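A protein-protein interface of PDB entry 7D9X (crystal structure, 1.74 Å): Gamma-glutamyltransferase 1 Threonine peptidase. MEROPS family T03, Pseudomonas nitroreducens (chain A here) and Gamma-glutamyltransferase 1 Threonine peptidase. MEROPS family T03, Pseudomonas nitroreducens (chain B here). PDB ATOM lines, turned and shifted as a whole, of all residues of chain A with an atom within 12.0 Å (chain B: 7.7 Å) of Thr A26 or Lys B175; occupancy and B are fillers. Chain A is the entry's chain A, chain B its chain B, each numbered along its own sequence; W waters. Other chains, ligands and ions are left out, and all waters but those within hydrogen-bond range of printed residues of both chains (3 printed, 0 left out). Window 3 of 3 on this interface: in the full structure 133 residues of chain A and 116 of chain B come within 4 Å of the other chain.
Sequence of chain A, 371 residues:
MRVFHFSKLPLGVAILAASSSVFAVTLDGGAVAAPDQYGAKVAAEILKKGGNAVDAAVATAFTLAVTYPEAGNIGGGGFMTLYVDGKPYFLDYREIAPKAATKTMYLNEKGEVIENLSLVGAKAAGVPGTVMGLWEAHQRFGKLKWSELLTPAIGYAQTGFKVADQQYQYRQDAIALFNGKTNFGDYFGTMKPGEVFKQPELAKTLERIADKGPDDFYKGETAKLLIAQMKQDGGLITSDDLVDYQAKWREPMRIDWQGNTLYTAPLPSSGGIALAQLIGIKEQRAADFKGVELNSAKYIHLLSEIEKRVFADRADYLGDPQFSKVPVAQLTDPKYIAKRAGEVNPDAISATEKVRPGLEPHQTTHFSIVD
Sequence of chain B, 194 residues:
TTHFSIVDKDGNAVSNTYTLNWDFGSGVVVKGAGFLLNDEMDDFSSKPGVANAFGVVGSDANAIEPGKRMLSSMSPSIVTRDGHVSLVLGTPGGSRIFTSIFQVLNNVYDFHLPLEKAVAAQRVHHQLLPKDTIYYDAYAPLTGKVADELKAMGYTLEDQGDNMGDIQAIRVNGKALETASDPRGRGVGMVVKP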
ATOM      1  N   THR A  26     -11.573 -19.255  26.448  1.00  0.00           N
ATOM      2  CA  THR A  26     -10.400 -19.337  25.562  1.00  0.00           C
ATOM      3  C   THR A  26      -9.200 -19.923  26.314  1.00  0.00           C
ATOM      4  O   THR A  26      -9.192 -21.110  26.639  1.00  0.00           O
ATOM      5  CB  THR A  26     -10.029 -17.957  24.972  1.00  0.00           C
ATOM      6  N   LEU A  27      -8.190 -19.098  26.595  1.00  0.00           N
ATOM      7  CA  LEU A  27      -6.971 -19.593  27.223  1.00  0.00           C
ATOM      8  C   LEU A  27      -7.072 -19.536  28.752  1.00  0.00           C
ATOM      9  O   LEU A  27      -7.892 -18.813  29.320  1.00  0.00           O
ATOM     10  CB  LEU A  27      -5.762 -18.769  26.754  1.00  0.00           C
ATOM     11  CG  LEU A  27      -5.495 -18.788  25.255  1.00  0.00           C
ATOM     12  CD1 LEU A  27      -4.222 -17.968  24.942  1.00  0.00           C
ATOM     13  CD2 LEU A  27      -5.340 -20.176  24.720  1.00  0.00           C
ATOM     14  N   ASP A  28      -6.198 -20.301  29.408  1.00  0.00           N
ATOM     15  CA  ASP A  28      -6.142 -20.312  30.865  1.00  0.00           C
ATOM     16  C   ASP A  28      -5.772 -18.956  31.440  1.00  0.00           C
ATOM     17  O   ASP A  28      -5.942 -18.734  32.644  1.00  0.00           O
ATOM     18  CB  ASP A  28      -5.117 -21.329  31.388  1.00  0.00           C
ATOM     19  CG  ASP A  28      -5.536 -22.768  31.175  1.00  0.00           C
ATOM     20  OD1 ASP A  28      -6.738 -23.007  30.951  1.00  0.00           O
ATOM     21  OD2 ASP A  28      -4.650 -23.658  31.255  1.00  0.00           O
ATOM     22  N   GLY A  29      -5.207 -18.075  30.622  1.00  0.00           N
ATOM     23  CA  GLY A  29      -4.742 -16.788  31.095  1.00  0.00           C
ATOM     24  C   GLY A  29      -3.882 -16.172  30.021  1.00  0.00           C
ATOM     25  O   GLY A  29      -3.934 -16.596  28.867  1.00  0.00           O
ATOM     26  N   GLY A  30      -3.096 -15.171  30.423  1.00  0.00           N
ATOM     27  CA  GLY A  30      -2.072 -14.593  29.587  1.00  0.00           C
ATOM     28  C   GLY A  30      -0.688 -14.984  30.070  1.00  0.00           C
ATOM     29  O   GLY A  30      -0.513 -15.694  31.053  1.00  0.00           O
ATOM     30  N   ALA A  31       0.315 -14.510  29.331  1.00  0.00           N
ATOM     31  CA  ALA A  31       1.688 -14.850  29.683  1.00  0.00           C
ATOM     32  C   ALA A  31       2.638 -13.814  29.109  1.00  0.00           C
ATOM     33  O   ALA A  31       2.329 -13.136  28.124  1.00  0.00           O
ATOM     34  CB  ALA A  31       2.076 -16.245  29.168  1.00  0.00           C
ATOM     35  N   TYR A  83      -0.888 -10.886  16.510  1.00  0.00           N
ATOM     36  CA  TYR A  83      -2.043 -11.691  16.125  1.00  0.00           C
ATOM     37  C   TYR A  83      -3.194 -11.220  17.004  1.00  0.00           C
ATOM     38  O   TYR A  83      -3.159 -11.386  18.227  1.00  0.00           O
ATOM     39  CB  TYR A  83      -1.759 -13.169  16.300  1.00  0.00           C
ATOM     40  CG  TYR A  83      -2.589 -14.066  15.419  1.00  0.00           C
ATOM     41  CD1 TYR A  83      -2.315 -14.188  14.071  1.00  0.00           C
ATOM     42  CD2 TYR A  83      -3.644 -14.805  15.945  1.00  0.00           C
ATOM     43  CE1 TYR A  83      -3.057 -15.043  13.266  1.00  0.00           C
ATOM     44  CE2 TYR A  83      -4.394 -15.647  15.152  1.00  0.00           C
ATOM     45  CZ  TYR A  83      -4.094 -15.757  13.810  1.00  0.00           C
ATOM     46  OH  TYR A  83      -4.829 -16.610  13.015  1.00  0.00           O
ATOM     47  N   VAL A  84      -4.193 -10.591  16.400  1.00  0.00           N
ATOM     48  CA  VAL A  84      -5.281  -9.970  17.154  1.00  0.00           C
ATOM     49  C   VAL A  84      -6.598 -10.420  16.549  1.00  0.00           C
ATOM     50  O   VAL A  84      -6.811 -10.267  15.343  1.00  0.00           O
ATOM     51  CB  VAL A  84      -5.183  -8.435  17.145  1.00  0.00           C
ATOM     52  CG1 VAL A  84      -6.321  -7.806  17.937  1.00  0.00           C
ATOM     53  CG2 VAL A  84      -3.842  -7.976  17.716  1.00  0.00           C
ATOM     54  N   ASP A  85      -7.465 -11.004  17.381  1.00  0.00           N
ATOM     55  CA  ASP A  85      -8.790 -11.452  16.945  1.00  0.00           C
ATOM     56  C   ASP A  85      -8.688 -12.296  15.678  1.00  0.00           C
ATOM     57  O   ASP A  85      -9.442 -12.115  14.718  1.00  0.00           O
ATOM     58  CB  ASP A  85      -9.709 -10.244  16.741  1.00  0.00           C
ATOM     59  CG  ASP A  85     -10.021  -9.524  18.045  1.00  0.00           C
ATOM     60  OD1 ASP A  85     -10.045 -10.199  19.093  1.00  0.00           O
ATOM     61  OD2 ASP A  85     -10.230  -8.289  18.028  1.00  0.00           O
ATOM     62  N   GLY A  86      -7.725 -13.219  15.674  1.00  0.00           N
ATOM     63  CA  GLY A  86      -7.573 -14.187  14.612  1.00  0.00           C
ATOM     64  C   GLY A  86      -6.928 -13.692  13.342  1.00  0.00           C
ATOM     65  O   GLY A  86      -6.974 -14.401  12.341  1.00  0.00           O
ATOM     66  N   ASP B   8      -2.219 -12.721  25.586  1.00  0.00           N
ATOM     67  CA  ASP B   8      -3.276 -12.407  26.555  1.00  0.00           C
ATOM     68  C   ASP B   8      -4.333 -13.504  26.579  1.00  0.00           C
ATOM     69  O   ASP B   8      -4.319 -14.441  25.778  1.00  0.00           O
ATOM     70  CB  ASP B   8      -3.911 -11.030  26.308  1.00  0.00           C
ATOM     71  CG  ASP B   8      -4.714 -10.935  25.013  1.00  0.00           C
ATOM     72  OD1 ASP B   8      -5.334 -11.932  24.553  1.00  0.00           O
ATOM     73  OD2 ASP B   8      -4.734  -9.820  24.436  1.00  0.00           O
ATOM     74  N   LYS B   9      -5.237 -13.396  27.562  1.00  0.00           N
ATOM     75  CA  LYS B   9      -6.206 -14.456  27.795  1.00  0.00           C
ATOM     76  C   LYS B   9      -7.206 -14.617  26.658  1.00  0.00           C
ATOM     77  O   LYS B   9      -7.892 -15.642  26.604  1.00  0.00           O
ATOM     78  CB  LYS B   9      -6.931 -14.177  29.117  1.00  0.00           C
ATOM     79  CG  LYS B   9      -7.721 -12.883  29.106  1.00  0.00           C
ATOM     80  CD  LYS B   9      -8.365 -12.632  30.460  1.00  0.00           C
ATOM     81  CE  LYS B   9      -9.185 -11.350  30.447  1.00  0.00           C
ATOM     82  NZ  LYS B   9      -8.326 -10.124  30.325  1.00  0.00           N
ATOM     83  N   ASP B  10      -7.306 -13.653  25.759  1.00  0.00           N
ATOM     84  CA  ASP B  10      -8.147 -13.764  24.579  1.00  0.00           C
ATOM     85  C   ASP B  10      -7.462 -14.460  23.411  1.00  0.00           C
ATOM     86  O   ASP B  10      -8.074 -14.611  22.347  1.00  0.00           O
ATOM     87  CB  ASP B  10      -8.601 -12.359  24.159  1.00  0.00           C
ATOM     88  CG  ASP B  10      -9.499 -11.722  25.196  1.00  0.00           C
ATOM     89  OD1 ASP B  10     -10.298 -12.466  25.795  1.00  0.00           O
ATOM     90  OD2 ASP B  10      -9.382 -10.498  25.428  1.00  0.00           O
ATOM     91  N   GLY B  11      -6.225 -14.898  23.576  1.00  0.00           N
ATOM     92  CA  GLY B  11      -5.495 -15.523  22.490  1.00  0.00           C
ATOM     93  C   GLY B  11      -4.790 -14.562  21.569  1.00  0.00           C
ATOM     94  O   GLY B  11      -4.269 -14.998  20.534  1.00  0.00           O
ATOM     95  N   ASN B  12      -4.786 -13.272  21.890  1.00  0.00           N
ATOM     96  CA  ASN B  12      -4.039 -12.294  21.123  1.00  0.00           C
ATOM     97  C   ASN B  12      -2.584 -12.330  21.539  1.00  0.00           C
ATOM     98  O   ASN B  12      -2.270 -12.667  22.673  1.00  0.00           O
ATOM     99  CB  ASN B  12      -4.587 -10.888  21.341  1.00  0.00           C
ATOM    100  CG  ASN B  12      -6.043 -10.772  20.980  1.00  0.00           C
ATOM    101  OD1 ASN B  12      -6.491 -11.320  19.974  1.00  0.00           O
ATOM    102  ND2 ASN B  12      -6.796 -10.063  21.806  1.00  0.00           N
ATOM    103  N   HIS B  84      -5.163 -20.335  15.500  1.00  0.00           N
ATOM    104  CA  HIS B  84      -4.894 -20.016  16.894  1.00  0.00           C
ATOM    105  C   HIS B  84      -3.388 -19.920  17.128  1.00  0.00           C
ATOM    106  O   HIS B  84      -2.614 -20.706  16.567  1.00  0.00           O
ATOM    107  CB  HIS B  84      -5.488 -21.076  17.815  1.00  0.00           C
ATOM    108  CG  HIS B  84      -6.984 -21.133  17.783  1.00  0.00           C
ATOM    109  ND1 HIS B  84      -7.679 -22.099  17.084  1.00  0.00           N
ATOM    110  CD2 HIS B  84      -7.919 -20.337  18.357  1.00  0.00           C
ATOM    111  CE1 HIS B  84      -8.977 -21.896  17.233  1.00  0.00           C
ATOM    112  NE2 HIS B  84      -9.150 -20.833  17.999  1.00  0.00           N
ATOM    113  N   ARG B 171       4.705 -20.754  24.533  1.00  0.00           N
ATOM    114  CA  ARG B 171       4.035 -21.821  23.810  1.00  0.00           C
ATOM    115  C   ARG B 171       2.606 -21.918  24.323  1.00  0.00           C
ATOM    116  O   ARG B 171       2.361 -21.842  25.539  1.00  0.00           O
ATOM    117  CB  ARG B 171       4.754 -23.172  23.974  1.00  0.00           C
ATOM    118  CG  ARG B 171       4.054 -24.311  23.262  1.00  0.00           C
ATOM    119  CD  ARG B 171       4.939 -25.583  23.175  1.00  0.00           C
ATOM    120  NE  ARG B 171       4.164 -26.752  22.759  1.00  0.00           N
ATOM    121  CZ  ARG B 171       3.598 -27.626  23.602  1.00  0.00           C
ATOM    122  N   VAL B 172       1.661 -22.040  23.389  1.00  0.00           N
ATOM    123  CA  VAL B 172       0.251 -22.235  23.704  1.00  0.00           C
ATOM    124  C   VAL B 172      -0.103 -23.656  23.295  1.00  0.00           C
ATOM    125  O   VAL B 172       0.045 -24.027  22.121  1.00  0.00           O
ATOM    126  CB  VAL B 172      -0.649 -21.220  22.991  1.00  0.00           C
ATOM    127  CG1 VAL B 172      -2.129 -21.470  23.367  1.00  0.00           C
ATOM    128  CG2 VAL B 172      -0.238 -19.812  23.373  1.00  0.00           C
ATOM    129  N   ASN B 173      -0.554 -24.443  24.265  1.00  0.00           N
ATOM    130  CA  ASN B 173      -0.843 -25.873  24.124  1.00  0.00           C
ATOM    131  C   ASN B 173      -2.320 -26.057  24.457  1.00  0.00           C
ATOM    132  O   ASN B 173      -2.679 -26.238  25.617  1.00  0.00           O
ATOM    133  CB  ASN B 173       0.047 -26.674  25.038  1.00  0.00           C
ATOM    134  CG  ASN B 173      -0.269 -28.147  25.020  1.00  0.00           C
ATOM    135  OD1 ASN B 173      -0.847 -28.664  24.057  1.00  0.00           O
ATOM    136  ND2 ASN B 173       0.120 -28.843  26.084  1.00  0.00           N
ATOM    137  N   GLY B 174      -3.169 -25.975  23.448  1.00  0.00           N
ATOM    138  CA  GLY B 174      -4.601 -25.899  23.722  1.00  0.00           C
ATOM    139  C   GLY B 174      -4.917 -24.620  24.472  1.00  0.00           C
ATOM    140  O   GLY B 174      -4.722 -23.508  23.970  1.00  0.00           O
ATOM    141  N   LYS B 175      -5.419 -24.743  25.705  1.00  0.00           N
ATOM    142  CA  LYS B 175      -5.694 -23.577  26.532  1.00  0.00           C
ATOM    143  C   LYS B 175      -4.562 -23.237  27.489  1.00  0.00           C
ATOM    144  O   LYS B 175      -4.641 -22.201  28.161  1.00  0.00           O
ATOM    145  CB  LYS B 175      -6.978 -23.786  27.348  1.00  0.00           C
ATOM    146  CG  LYS B 175      -8.236 -23.992  26.515  1.00  0.00           C
ATOM    147  CD  LYS B 175      -9.484 -24.038  27.404  1.00  0.00           C
ATOM    148  CE  LYS B 175     -10.762 -23.750  26.622  1.00  0.00           C
ATOM    149  N   ALA B 176      -3.539 -24.080  27.577  1.00  0.00           N
ATOM    150  CA  ALA B 176      -2.464 -23.926  28.545  1.00  0.00           C
ATOM    151  C   ALA B 176      -1.317 -23.105  27.957  1.00  0.00           C
ATOM    152  O   ALA B 176      -1.009 -23.217  26.767  1.00  0.00           O
ATOM    153  CB  ALA B 176      -1.912 -25.300  28.970  1.00  0.00           C
ATOM    154  N   LEU B 177      -0.658 -22.329  28.814  1.00  0.00           N
ATOM    155  CA  LEU B 177       0.458 -21.479  28.415  1.00  0.00           C
ATOM    156  C   LEU B 177       1.740 -21.909  29.122  1.00  0.00           C
ATOM    157  O   LEU B 177       1.722 -22.314  30.287  1.00  0.00           O
ATOM    158  CB  LEU B 177       0.151 -20.007  28.717  1.00  0.00           C
ATOM    159  CG  LEU B 177      -0.981 -19.436  27.854  1.00  0.00           C
ATOM    160  CD2 LEU B 177      -0.662 -18.070  27.333  1.00  0.00           C
ATOM    161  N   GLU B 178       2.853 -21.828  28.394  1.00  0.00           N
ATOM    162  CA  GLU B 178       4.191 -22.150  28.875  1.00  0.00           C
ATOM    163  C   GLU B 178       5.114 -21.027  28.427  1.00  0.00           C
ATOM    164  O   GLU B 178       4.969 -20.527  27.315  1.00  0.00           O
ATOM    165  CB  GLU B 178       4.668 -23.498  28.295  1.00  0.00           C
ATOM    166  CG  GLU B 178       6.024 -23.962  28.765  1.00  0.00           C
ATOM    167  CD  GLU B 178       6.291 -25.446  28.407  1.00  0.00           C
ATOM    168  N   VAL B 191       3.122 -16.837  33.727  1.00  0.00           N
ATOM    169  CA  VAL B 191       1.747 -17.043  33.276  1.00  0.00           C
ATOM    170  C   VAL B 191       0.832 -16.286  34.232  1.00  0.00           C
ATOM    171  O   VAL B 191       1.004 -16.342  35.459  1.00  0.00           O
ATOM    172  CB  VAL B 191       1.397 -18.539  33.226  1.00  0.00           C
ATOM    173  CG1 VAL B 191      -0.087 -18.721  32.935  1.00  0.00           C
ATOM    174  CG2 VAL B 191       2.246 -19.262  32.192  1.00  0.00           C
HETATM  175  O   HOH W   1      -1.793 -22.647  31.548  1.00  0.00           O
HETATM  176  O   HOH W   2      -6.315 -13.851  18.041  1.00  0.00           O
HETATM  177  O   HOH W   3      -9.514 -16.472  28.878  1.00  0.00           O
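The backbone NH (N) of Asp A85 sits at hydrogen-bond distance from the side-chain amide oxygen (OD1) of Asn B12 (2.8 Å). N of Leu A27 lies within hydrogen-bond range of O of Lys B9 (3.5 Å). The backbone carbonyl oxygen (O) of Lys B175 sits at hydrogen-bond distance from the backbone NH (N) of Asp A28, 2.8 Å away.
The side-chain carboxylate (OD1) of Asp B8 is in hydrogen-bond range of the backbone NH (N) of Asp B10, at 2.9 Å. The side-chain hydroxyl (OH) of Tyr A83 lies within hydrogen-bond range of the backbone carbonyl oxygen (O) of Gly A86, at 3.2 Å. The backbone NH (N) of Gly B11 sits at hydrogen-bond distance from the side-chain carboxylate (OD1) of Asp B8, at 3.2 Å. The side-chain carboxylate (OD1) of Asp B8 sits at hydrogen-bond distance from the backbone NH (N) of Asn B12 (3.0 Å).
Among the printed residues, pairs that only touch across the chains: Thr A26 with Lys B9 (3.5 Å), Thr A26 with Lys B175 (3.0 Å), Leu A27 with Asp B8 (3.6 Å), Leu A27 with Gly B11 (3.7 Å), Leu A27 with Val B172 (3.7 Å), Leu A27 with Gly B174 (3.5 Å), Leu A27 with Lys B175 (3.6 Å), Asp A28 with Ala B176 (3.5 Å), Gly A29 with Asp B8 (3.8 Å), Gly A29 with Lys B9 (3.3 Å), Gly A29 with Leu B177 (3.9 Å), Gly A30 with Asp B8 (3.9 Å), Gly A30 with Lys B9 (3.9 Å), Gly A30 with Val B191 (3.4 Å), Ala A31 with Leu B177 (3.8 Å), Tyr A83 with Asn B12 (3.2 Å) and Val A84 with Asn B12 (3.4 Å).
Of the printed residues of chain B, Thr A26 touches Lys B9 (3.5 Å) and Lys B175 (3.0 Å). Printed residues of chain B within 4 Å of Asp A28: Lys B175 (2.8 Å) and Ala B176 (3.5 Å). Printed residues of chain B within 4 Å of Gly A29: Asp B8, Lys B9 and Leu B177. Of the printed residues of chain B, Val A84 touches Asn B12. Of the printed residues of chain A, Lys B9 touches Thr A26, Leu A27, Gly A29 and Gly A30. No residue of chain A comes within 4 Å of Asp B10. Of the printed residues of chain A, Gly B11 touches Leu A27 (3.7 Å). His B84 touches none of the printed residues of chain A. Val B172 touches one residue of chain A. No residue of chain A comes within 4 Å of Asn B173. Of chain A, only Leu A27 (3.5 Å) comes within 4 Å of Gly B174. Lys B175 touches just these residues of chain A: Thr A26, Leu A27 and Asp A28. Of the printed residues of chain A, Leu B177 touches Gly A29 (3.9 Å) and Ala A31 (3.8 Å). Glu B178 touches none of the printed residues of chain A. Printed residues of chain A within 4 Å of Val B191: Gly A30. The nearest residue of chain B that does not touch Thr A26 is Asp B10 (4.6 Å). The nearest printed residue of chain A that does not touch Asp B8 is Ala A31 (4.9 Å).
Of the 15 printed residues of chain B, 10 touch a printed residue of chain A. Printed residues of chain B that touch a printed residue of chain A: Asp B8, Lys B9, Gly B11, Asn B12, Val B172, Gly B174, Lys B175, Ala B176, Leu B177 and Val B191. Along chain B the printed residues that touch a printed residue of chain A span positions 8 to 191. Of the 10 printed residues of chain A, 9 touch a printed residue of chain B. Among the printed residues, 20 pairs touch across the chains. Among the printed residues, no Asp or Glu carboxylate lies within 4 Å of a Lys or Arg side-chain nitrogen of the other chain.
Water W2 lies within hydrogen-bond range of N of Gly A86 (2.8 Å), N of Asp A85 (3.1 Å), OD1 of Asn B12 (3.2 Å) and O of Gly B11 (3.4 Å). Water W3 bridges the backbone carbonyl oxygen of Leu A27 (2.9 Å) and the backbone carbonyl oxygen of Lys B9 (2.9 Å). Water W1 bridges N of Leu B177 (3.0 Å) and OD2 of Asp A28 (3.0 Å).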
